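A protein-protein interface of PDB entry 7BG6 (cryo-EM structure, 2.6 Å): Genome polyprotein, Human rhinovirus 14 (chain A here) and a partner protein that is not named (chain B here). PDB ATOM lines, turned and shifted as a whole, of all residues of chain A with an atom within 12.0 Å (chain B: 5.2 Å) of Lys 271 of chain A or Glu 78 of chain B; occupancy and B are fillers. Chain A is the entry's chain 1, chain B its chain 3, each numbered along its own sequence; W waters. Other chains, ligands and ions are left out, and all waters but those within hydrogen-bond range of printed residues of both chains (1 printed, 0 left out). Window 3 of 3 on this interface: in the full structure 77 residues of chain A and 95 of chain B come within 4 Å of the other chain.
The guanidinium group of Arg 266 of chain A sits at hydrogen-bond distance from the backbone carbonyl oxygen of Gly 82 of chain B (2.8 Å).
O of Ile 270 of chain A is in hydrogen-bond range of N of Gly 82 of chain B, at 2.8 Å.
OE1 of Glu 78 of chain B lies within salt-bridge range of NZ of Lys 271 of chain A (3.95 Å).
The side-chain amide nitrogen of Gln 79 of chain B lies within hydrogen-bond range of the backbone carbonyl oxygen of Lys 271 of chain A (3.3 Å).
The backbone carbonyl oxygen (O) of Ser 272 of chain A sits close to the backbone carbonyl oxygen (O) of Gly 82 of chain B (2.7 Å).
OH of Tyr 273 of chain A sits at hydrogen-bond distance from NE2 of Gln 79 of chain B (2.9 Å).
The backbone carbonyl oxygen (O) of Ile 270 of chain A lies within hydrogen-bond range of the guanidinium group (NH1) of Arg 266 of chain A.
The guanidinium group of Arg 266 of chain A is in hydrogen-bond range of the backbone carbonyl oxygen of Ser 272 of chain A.
OG of Ser 272 of chain A sits at hydrogen-bond distance from O of Asp 269 of chain A (3.3 Å).
The backbone carbonyl oxygen of Glu 78 of chain B is in hydrogen-bond range of the backbone NH of Tyr 191 of chain B (2.9 Å).
The side-chain amide nitrogen (NE2) of Gln 79 of chain B lies within hydrogen-bond range of the backbone carbonyl oxygen (O) of Phe 81 of chain B, 3.2 Å away.
The backbone NH of Cys 189 of chain B is in hydrogen-bond range of the backbone carbonyl oxygen of Phe 81 of chain B (3.1 Å).
Among the printed residues, merely in contact across the chains: Ile 270 of chain A with Phe 81 of chain B (3.4 Å), Ile 270 of chain A with Val 80 of chain B (3.5 Å), Lys 271 of chain A with Gly 82 of chain B (3.7 Å), Tyr 273 of chain A with Gly 82 of chain B (3.9 Å) and Tyr 273 of chain A with Trp 190 of chain B (3.9 Å).
Of chain B, only Glu 78 (3.95 Å), Gln 79 (3.3 Å) and Gly 82 (3.7 Å) come within 4 Å of Lys 271 of chain A.
Glu 78 of chain B touches one residue of chain A.
No residue of chain A comes within 4 Å of Asn 77 of chain B.
Of chain A, only Lys 271 and Tyr 273 come within 4 Å of Gln 79 of chain B.
Of chain A, only Arg 266, Ile 270, Lys 271, Ser 272 and Tyr 273 come within 4 Å of Gly 82 of chain B.
Of chain A, only Tyr 273 (3.9 Å) comes within 4 Å of Trp 190 of chain B.
Of the printed residues of chain B, Arg 266 of chain A touches Gly 82 (2.8 Å).
Of the printed residues of chain B, Ser 272 of chain A touches Gly 82.
Asp 269 of chain A touches none of the printed residues of chain B.
The nearest residue of chain A that does not touch Glu 78 of chain B is Ile 270 of chain A (8.9 Å).
Printed residues of chain A that touch a printed residue of chain B: Arg 266, Ile 270, Lys 271, Ser 272 and Tyr 273.
Among the printed residues, 11 pairs touch across the chains.
Among the printed residues, Asp or Glu carboxylates within 4 Å of a Lys or Arg side-chain nitrogen of the other chain: Lys 271 of chain A with Glu 78 of chain B.
Water W1 bridges O of Lys 271 of chain A (2.4 Å) and OE1 of Gln 79 of chain B (3.2 Å).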
ATOM      1  N   LYS A 264      -2.279  -1.765   3.651  1.00  0.00           N
ATOM      2  CA  LYS A 264      -1.420  -2.300   2.607  1.00  0.00           C
ATOM      3  C   LYS A 264      -0.216  -1.384   2.402  1.00  0.00           C
ATOM      4  O   LYS A 264      -0.288  -0.442   1.615  1.00  0.00           O
ATOM      5  CB  LYS A 264      -2.238  -2.393   1.315  1.00  0.00           C
ATOM      6  CG  LYS A 264      -2.000  -3.626   0.454  1.00  0.00           C
ATOM      7  CD  LYS A 264      -2.863  -3.633  -0.791  1.00  0.00           C
ATOM      8  CE  LYS A 264      -3.032  -5.007  -1.402  1.00  0.00           C
ATOM      9  NZ  LYS A 264      -3.926  -5.868  -0.590  1.00  0.00           N
ATOM     10  N   LYS A 265       0.895  -1.689   3.086  1.00  0.00           N
ATOM     11  CA  LYS A 265       2.085  -0.850   3.064  1.00  0.00           C
ATOM     12  C   LYS A 265       2.509  -0.570   1.623  1.00  0.00           C
ATOM     13  O   LYS A 265       2.433  -1.446   0.762  1.00  0.00           O
ATOM     14  CB  LYS A 265       3.232  -1.476   3.865  1.00  0.00           C
ATOM     15  CG  LYS A 265       4.353  -0.510   4.233  1.00  0.00           C
ATOM     16  CD  LYS A 265       5.692  -1.173   4.465  1.00  0.00           C
ATOM     17  CE  LYS A 265       6.835  -0.180   4.506  1.00  0.00           C
ATOM     18  NZ  LYS A 265       8.139  -0.847   4.732  1.00  0.00           N
ATOM     19  N   ARG A 266       2.961   0.668   1.389  1.00  0.00           N
ATOM     20  CA  ARG A 266       3.336   1.151   0.070  1.00  0.00           C
ATOM     21  C   ARG A 266       4.683   0.570  -0.343  1.00  0.00           C
ATOM     22  O   ARG A 266       5.475   0.148   0.497  1.00  0.00           O
ATOM     23  CB  ARG A 266       3.487   2.676   0.087  1.00  0.00           C
ATOM     24  CG  ARG A 266       2.180   3.456   0.100  1.00  0.00           C
ATOM     25  CD  ARG A 266       2.484   4.911   0.402  1.00  0.00           C
ATOM     26  NE  ARG A 266       1.327   5.793   0.327  1.00  0.00           N
ATOM     27  CZ  ARG A 266       1.007   6.540  -0.724  1.00  0.00           C
ATOM     28  NH1 ARG A 266       1.756   6.522  -1.814  1.00  0.00           N
ATOM     29  NH2 ARG A 266      -0.067   7.308  -0.682  1.00  0.00           N
ATOM     30  N   LYS A 267       4.915   0.560  -1.661  1.00  0.00           N
ATOM     31  CA  LYS A 267       6.252   0.469  -2.222  1.00  0.00           C
ATOM     32  C   LYS A 267       6.749   1.893  -2.453  1.00  0.00           C
ATOM     33  O   LYS A 267       6.315   2.562  -3.390  1.00  0.00           O
ATOM     34  CB  LYS A 267       6.241  -0.335  -3.527  1.00  0.00           C
ATOM     35  CG  LYS A 267       5.803  -1.789  -3.410  1.00  0.00           C
ATOM     36  CD  LYS A 267       6.789  -2.667  -2.666  1.00  0.00           C
ATOM     37  CE  LYS A 267       6.331  -4.105  -2.550  1.00  0.00           C
ATOM     38  NZ  LYS A 267       7.291  -4.925  -1.776  1.00  0.00           N
ATOM     39  N   GLY A 268       7.640   2.353  -1.568  1.00  0.00           N
ATOM     40  CA  GLY A 268       8.126   3.722  -1.601  1.00  0.00           C
ATOM     41  C   GLY A 268       7.426   4.596  -0.564  1.00  0.00           C
ATOM     42  O   GLY A 268       6.727   4.091   0.313  1.00  0.00           O
ATOM     43  N   ASP A 269       7.615   5.916  -0.695  1.00  0.00           N
ATOM     44  CA  ASP A 269       7.170   6.881   0.298  1.00  0.00           C
ATOM     45  C   ASP A 269       5.708   7.254   0.061  1.00  0.00           C
ATOM     46  O   ASP A 269       5.037   6.667  -0.787  1.00  0.00           O
ATOM     47  CB  ASP A 269       8.088   8.107   0.323  1.00  0.00           C
ATOM     48  CG  ASP A 269       9.509   7.803   0.769  1.00  0.00           C
ATOM     49  OD1 ASP A 269      10.443   8.366   0.164  1.00  0.00           O
ATOM     50  OD2 ASP A 269       9.673   7.013   1.722  1.00  0.00           O
ATOM     51  N   ILE A 270       5.239   8.250   0.825  1.00  0.00           N
ATOM     52  CA  ILE A 270       3.868   8.735   0.788  1.00  0.00           C
ATOM     53  C   ILE A 270       3.611   9.455  -0.538  1.00  0.00           C
ATOM     54  O   ILE A 270       2.467   9.770  -0.863  1.00  0.00           O
ATOM     55  CB  ILE A 270       3.584   9.637   2.012  1.00  0.00           C
ATOM     56  CG1 ILE A 270       2.085   9.878   2.221  1.00  0.00           C
ATOM     57  CG2 ILE A 270       4.374  10.938   1.937  1.00  0.00           C
ATOM     58  CD1 ILE A 270       1.741  10.631   3.488  1.00  0.00           C
ATOM     59  N   LYS A 271       4.685   9.691  -1.301  1.00  0.00           N
ATOM     60  CA  LYS A 271       4.627  10.477  -2.524  1.00  0.00           C
ATOM     61  C   LYS A 271       4.451   9.568  -3.739  1.00  0.00           C
ATOM     62  O   LYS A 271       4.178  10.053  -4.836  1.00  0.00           O
ATOM     63  CB  LYS A 271       5.900  11.319  -2.674  1.00  0.00           C
ATOM     64  CG  LYS A 271       6.174  12.313  -1.553  1.00  0.00           C
ATOM     65  CD  LYS A 271       7.521  12.994  -1.681  1.00  0.00           C
ATOM     66  CE  LYS A 271       7.877  13.844  -0.480  1.00  0.00           C
ATOM     67  NZ  LYS A 271       9.202  14.488  -0.637  1.00  0.00           N
ATOM     68  N   SER A 272       4.607   8.253  -3.534  1.00  0.00           N
ATOM     69  CA  SER A 272       4.626   7.290  -4.626  1.00  0.00           C
ATOM     70  C   SER A 272       3.216   7.055  -5.166  1.00  0.00           C
ATOM     71  O   SER A 272       2.231   7.284  -4.469  1.00  0.00           O
ATOM     72  CB  SER A 272       5.278   5.996  -4.203  1.00  0.00           C
ATOM     73  OG  SER A 272       4.340   5.132  -3.577  1.00  0.00           O
ATOM     74  N   TYR A 273       3.146   6.588  -6.418  1.00  0.00           N
ATOM     75  CA  TYR A 273       1.887   6.261  -7.067  1.00  0.00           C
ATOM     76  C   TYR A 273       1.803   4.746  -7.291  1.00  0.00           C
ATOM     77  O   TYR A 273       2.813   4.042  -7.307  1.00  0.00           O
ATOM     78  CB  TYR A 273       1.745   7.028  -8.386  1.00  0.00           C
ATOM     79  CG  TYR A 273       1.825   8.529  -8.260  1.00  0.00           C
ATOM     80  CD1 TYR A 273       2.989   9.211  -8.580  1.00  0.00           C
ATOM     81  CD2 TYR A 273       0.738   9.271  -7.821  1.00  0.00           C
ATOM     82  CE1 TYR A 273       3.073  10.590  -8.467  1.00  0.00           C
ATOM     83  CE2 TYR A 273       0.805  10.651  -7.705  1.00  0.00           C
ATOM     84  CZ  TYR A 273       1.976  11.312  -8.030  1.00  0.00           C
ATOM     85  OH  TYR A 273       2.051  12.671  -7.917  1.00  0.00           O
ATOM     86  OXT TYR A 273       0.716   4.193  -7.461  1.00  0.00           O
ATOM     87  N   ARG B  75       8.961  24.372   3.282  1.00  0.00           N
ATOM     88  CA  ARG B  75       9.155  23.597   2.067  1.00  0.00           C
ATOM     89  C   ARG B  75       8.367  24.258   0.939  1.00  0.00           C
ATOM     90  O   ARG B  75       7.147  24.391   1.024  1.00  0.00           O
ATOM     91  CB  ARG B  75       8.696  22.147   2.255  1.00  0.00           C
ATOM     92  CG  ARG B  75       9.323  21.424   3.440  1.00  0.00           C
ATOM     93  CD  ARG B  75      10.745  20.948   3.210  1.00  0.00           C
ATOM     94  NE  ARG B  75      11.230  20.172   4.344  1.00  0.00           N
ATOM     95  CZ  ARG B  75      11.110  18.853   4.474  1.00  0.00           C
ATOM     96  NH1 ARG B  75      10.518  18.140   3.530  1.00  0.00           N
ATOM     97  NH2 ARG B  75      11.583  18.252   5.550  1.00  0.00           N
ATOM     98  N   GLN B  76       9.087  24.684  -0.105  1.00  0.00           N
ATOM     99  CA  GLN B  76       8.471  25.255  -1.290  1.00  0.00           C
ATOM    100  C   GLN B  76       8.411  24.187  -2.378  1.00  0.00           C
ATOM    101  O   GLN B  76       9.241  23.279  -2.400  1.00  0.00           O
ATOM    102  CB  GLN B  76       9.271  26.460  -1.788  1.00  0.00           C
ATOM    103  CG  GLN B  76       9.259  27.649  -0.838  1.00  0.00           C
ATOM    104  CD  GLN B  76       9.856  28.894  -1.450  1.00  0.00           C
ATOM    105  OE1 GLN B  76       9.939  29.038  -2.668  1.00  0.00           O
ATOM    106  NE2 GLN B  76      10.269  29.817  -0.598  1.00  0.00           N
ATOM    107  N   ASN B  77       7.414  24.314  -3.265  1.00  0.00           N
ATOM    108  CA  ASN B  77       7.299  23.533  -4.489  1.00  0.00           C
ATOM    109  C   ASN B  77       7.742  22.088  -4.255  1.00  0.00           C
ATOM    110  O   ASN B  77       8.663  21.600  -4.908  1.00  0.00           O
ATOM    111  CB  ASN B  77       8.008  24.214  -5.666  1.00  0.00           C
ATOM    112  CG  ASN B  77       9.395  24.728  -5.335  1.00  0.00           C
ATOM    113  OD1 ASN B  77      10.283  23.959  -4.968  1.00  0.00           O
ATOM    114  ND2 ASN B  77       9.597  26.027  -5.473  1.00  0.00           N
ATOM    115  N   GLU B  78       7.061  21.412  -3.321  1.00  0.00           N
ATOM    116  CA  GLU B  78       7.398  20.054  -2.927  1.00  0.00           C
ATOM    117  C   GLU B  78       6.112  19.260  -2.701  1.00  0.00           C
ATOM    118  O   GLU B  78       5.074  19.835  -2.381  1.00  0.00           O
ATOM    119  CB  GLU B  78       8.287  20.076  -1.681  1.00  0.00           C
ATOM    120  CG  GLU B  78       8.752  18.702  -1.228  1.00  0.00           C
ATOM    121  CD  GLU B  78       9.781  18.707  -0.111  1.00  0.00           C
ATOM    122  OE1 GLU B  78       9.511  18.097   0.943  1.00  0.00           O
ATOM    123  OE2 GLU B  78      10.855  19.314  -0.300  1.00  0.00           O
ATOM    124  N   GLN B  79       6.203  17.935  -2.866  1.00  0.00           N
ATOM    125  CA  GLN B  79       5.054  17.049  -2.776  1.00  0.00           C
ATOM    126  C   GLN B  79       4.733  16.749  -1.314  1.00  0.00           C
ATOM    127  O   GLN B  79       5.632  16.576  -0.493  1.00  0.00           O
ATOM    128  CB  GLN B  79       5.305  15.760  -3.561  1.00  0.00           C
ATOM    129  CG  GLN B  79       4.034  14.981  -3.874  1.00  0.00           C
ATOM    130  CD  GLN B  79       4.235  13.891  -4.900  1.00  0.00           C
ATOM    131  OE1 GLN B  79       5.342  13.654  -5.380  1.00  0.00           O
ATOM    132  NE2 GLN B  79       3.152  13.215  -5.246  1.00  0.00           N
ATOM    133  N   VAL B  80       3.430  16.683  -1.019  1.00  0.00           N
ATOM    134  CA  VAL B  80       2.920  16.360   0.303  1.00  0.00           C
ATOM    135  C   VAL B  80       2.589  14.869   0.341  1.00  0.00           C
ATOM    136  O   VAL B  80       3.093  14.143   1.195  1.00  0.00           O
ATOM    137  CB  VAL B  80       1.703  17.237   0.662  1.00  0.00           C
ATOM    138  CG1 VAL B  80       1.028  16.788   1.949  1.00  0.00           C
ATOM    139  CG2 VAL B  80       2.071  18.712   0.738  1.00  0.00           C
ATOM    140  N   PHE B  81       1.735  14.431  -0.594  1.00  0.00           N
ATOM    141  CA  PHE B  81       1.410  13.024  -0.761  1.00  0.00           C
ATOM    142  C   PHE B  81       1.108  12.733  -2.229  1.00  0.00           C
ATOM    143  O   PHE B  81       0.928  13.649  -3.029  1.00  0.00           O
ATOM    144  CB  PHE B  81       0.250  12.610   0.153  1.00  0.00           C
ATOM    145  CG  PHE B  81      -1.115  13.091  -0.271  1.00  0.00           C
ATOM    146  CD1 PHE B  81      -1.724  14.157   0.374  1.00  0.00           C
ATOM    147  CD2 PHE B  81      -1.800  12.471  -1.308  1.00  0.00           C
ATOM    148  CE1 PHE B  81      -2.982  14.598  -0.014  1.00  0.00           C
ATOM    149  CE2 PHE B  81      -3.054  12.916  -1.700  1.00  0.00           C
ATOM    150  CZ  PHE B  81      -3.640  13.980  -1.054  1.00  0.00           C
ATOM    151  N   GLY B  82       1.055  11.437  -2.558  1.00  0.00           N
ATOM    152  CA  GLY B  82       0.649  10.964  -3.870  1.00  0.00           C
ATOM    153  C   GLY B  82       0.028   9.573  -3.780  1.00  0.00           C
ATOM    154  O   GLY B  82       0.481   8.741  -2.996  1.00  0.00           O
ATOM    155  N   CYS B 189      -0.838  16.050  -3.732  1.00  0.00           N
ATOM    156  CA  CYS B 189      -0.892  17.316  -3.020  1.00  0.00           C
ATOM    157  C   CYS B 189       0.509  17.916  -2.961  1.00  0.00           C
ATOM    158  O   CYS B 189       1.490  17.202  -2.768  1.00  0.00           O
ATOM    159  CB  CYS B 189      -1.439  17.136  -1.610  1.00  0.00           C
ATOM    160  SG  CYS B 189      -1.742  18.702  -0.748  1.00  0.00           S
ATOM    161  N   TRP B 190       0.575  19.240  -3.138  1.00  0.00           N
ATOM    162  CA  TRP B 190       1.836  19.959  -3.216  1.00  0.00           C
ATOM    163  C   TRP B 190       1.759  21.211  -2.350  1.00  0.00           C
ATOM    164  O   TRP B 190       0.670  21.688  -2.036  1.00  0.00           O
ATOM    165  CB  TRP B 190       2.157  20.314  -4.674  1.00  0.00           C
ATOM    166  CG  TRP B 190       2.026  19.157  -5.615  1.00  0.00           C
ATOM    167  CD1 TRP B 190       0.873  18.647  -6.135  1.00  0.00           C
ATOM    168  CD2 TRP B 190       3.095  18.349  -6.141  1.00  0.00           C
ATOM    169  NE1 TRP B 190       1.147  17.579  -6.943  1.00  0.00           N
ATOM    170  CE2 TRP B 190       2.500  17.373  -6.970  1.00  0.00           C
ATOM    171  CE3 TRP B 190       4.487  18.356  -5.997  1.00  0.00           C
ATOM    172  CZ2 TRP B 190       3.253  16.416  -7.650  1.00  0.00           C
ATOM    173  CZ3 TRP B 190       5.230  17.408  -6.666  1.00  0.00           C
ATOM    174  CH2 TRP B 190       4.619  16.450  -7.479  1.00  0.00           C
ATOM    175  N   TYR B 191       2.932  21.728  -1.969  1.00  0.00           N
ATOM    176  CA  TYR B 191       3.020  23.027  -1.327  1.00  0.00           C
ATOM    177  C   TYR B 191       2.826  24.105  -2.387  1.00  0.00           C
ATOM    178  O   TYR B 191       3.611  24.204  -3.329  1.00  0.00           O
ATOM    179  CB  TYR B 191       4.354  23.182  -0.591  1.00  0.00           C
ATOM    180  CG  TYR B 191       4.536  22.252   0.581  1.00  0.00           C
ATOM    181  CD1 TYR B 191       5.334  21.124   0.481  1.00  0.00           C
ATOM    182  CD2 TYR B 191       3.904  22.495   1.791  1.00  0.00           C
ATOM    183  CE1 TYR B 191       5.503  20.261   1.552  1.00  0.00           C
ATOM    184  CE2 TYR B 191       4.061  21.643   2.872  1.00  0.00           C
ATOM    185  CZ  TYR B 191       4.863  20.522   2.752  1.00  0.00           C
ATOM    186  OH  TYR B 191       5.025  19.677   3.811  1.00  0.00           O
HETATM  187  O   HOH W   1       5.595  10.750  -6.664  1.00  0.00           O
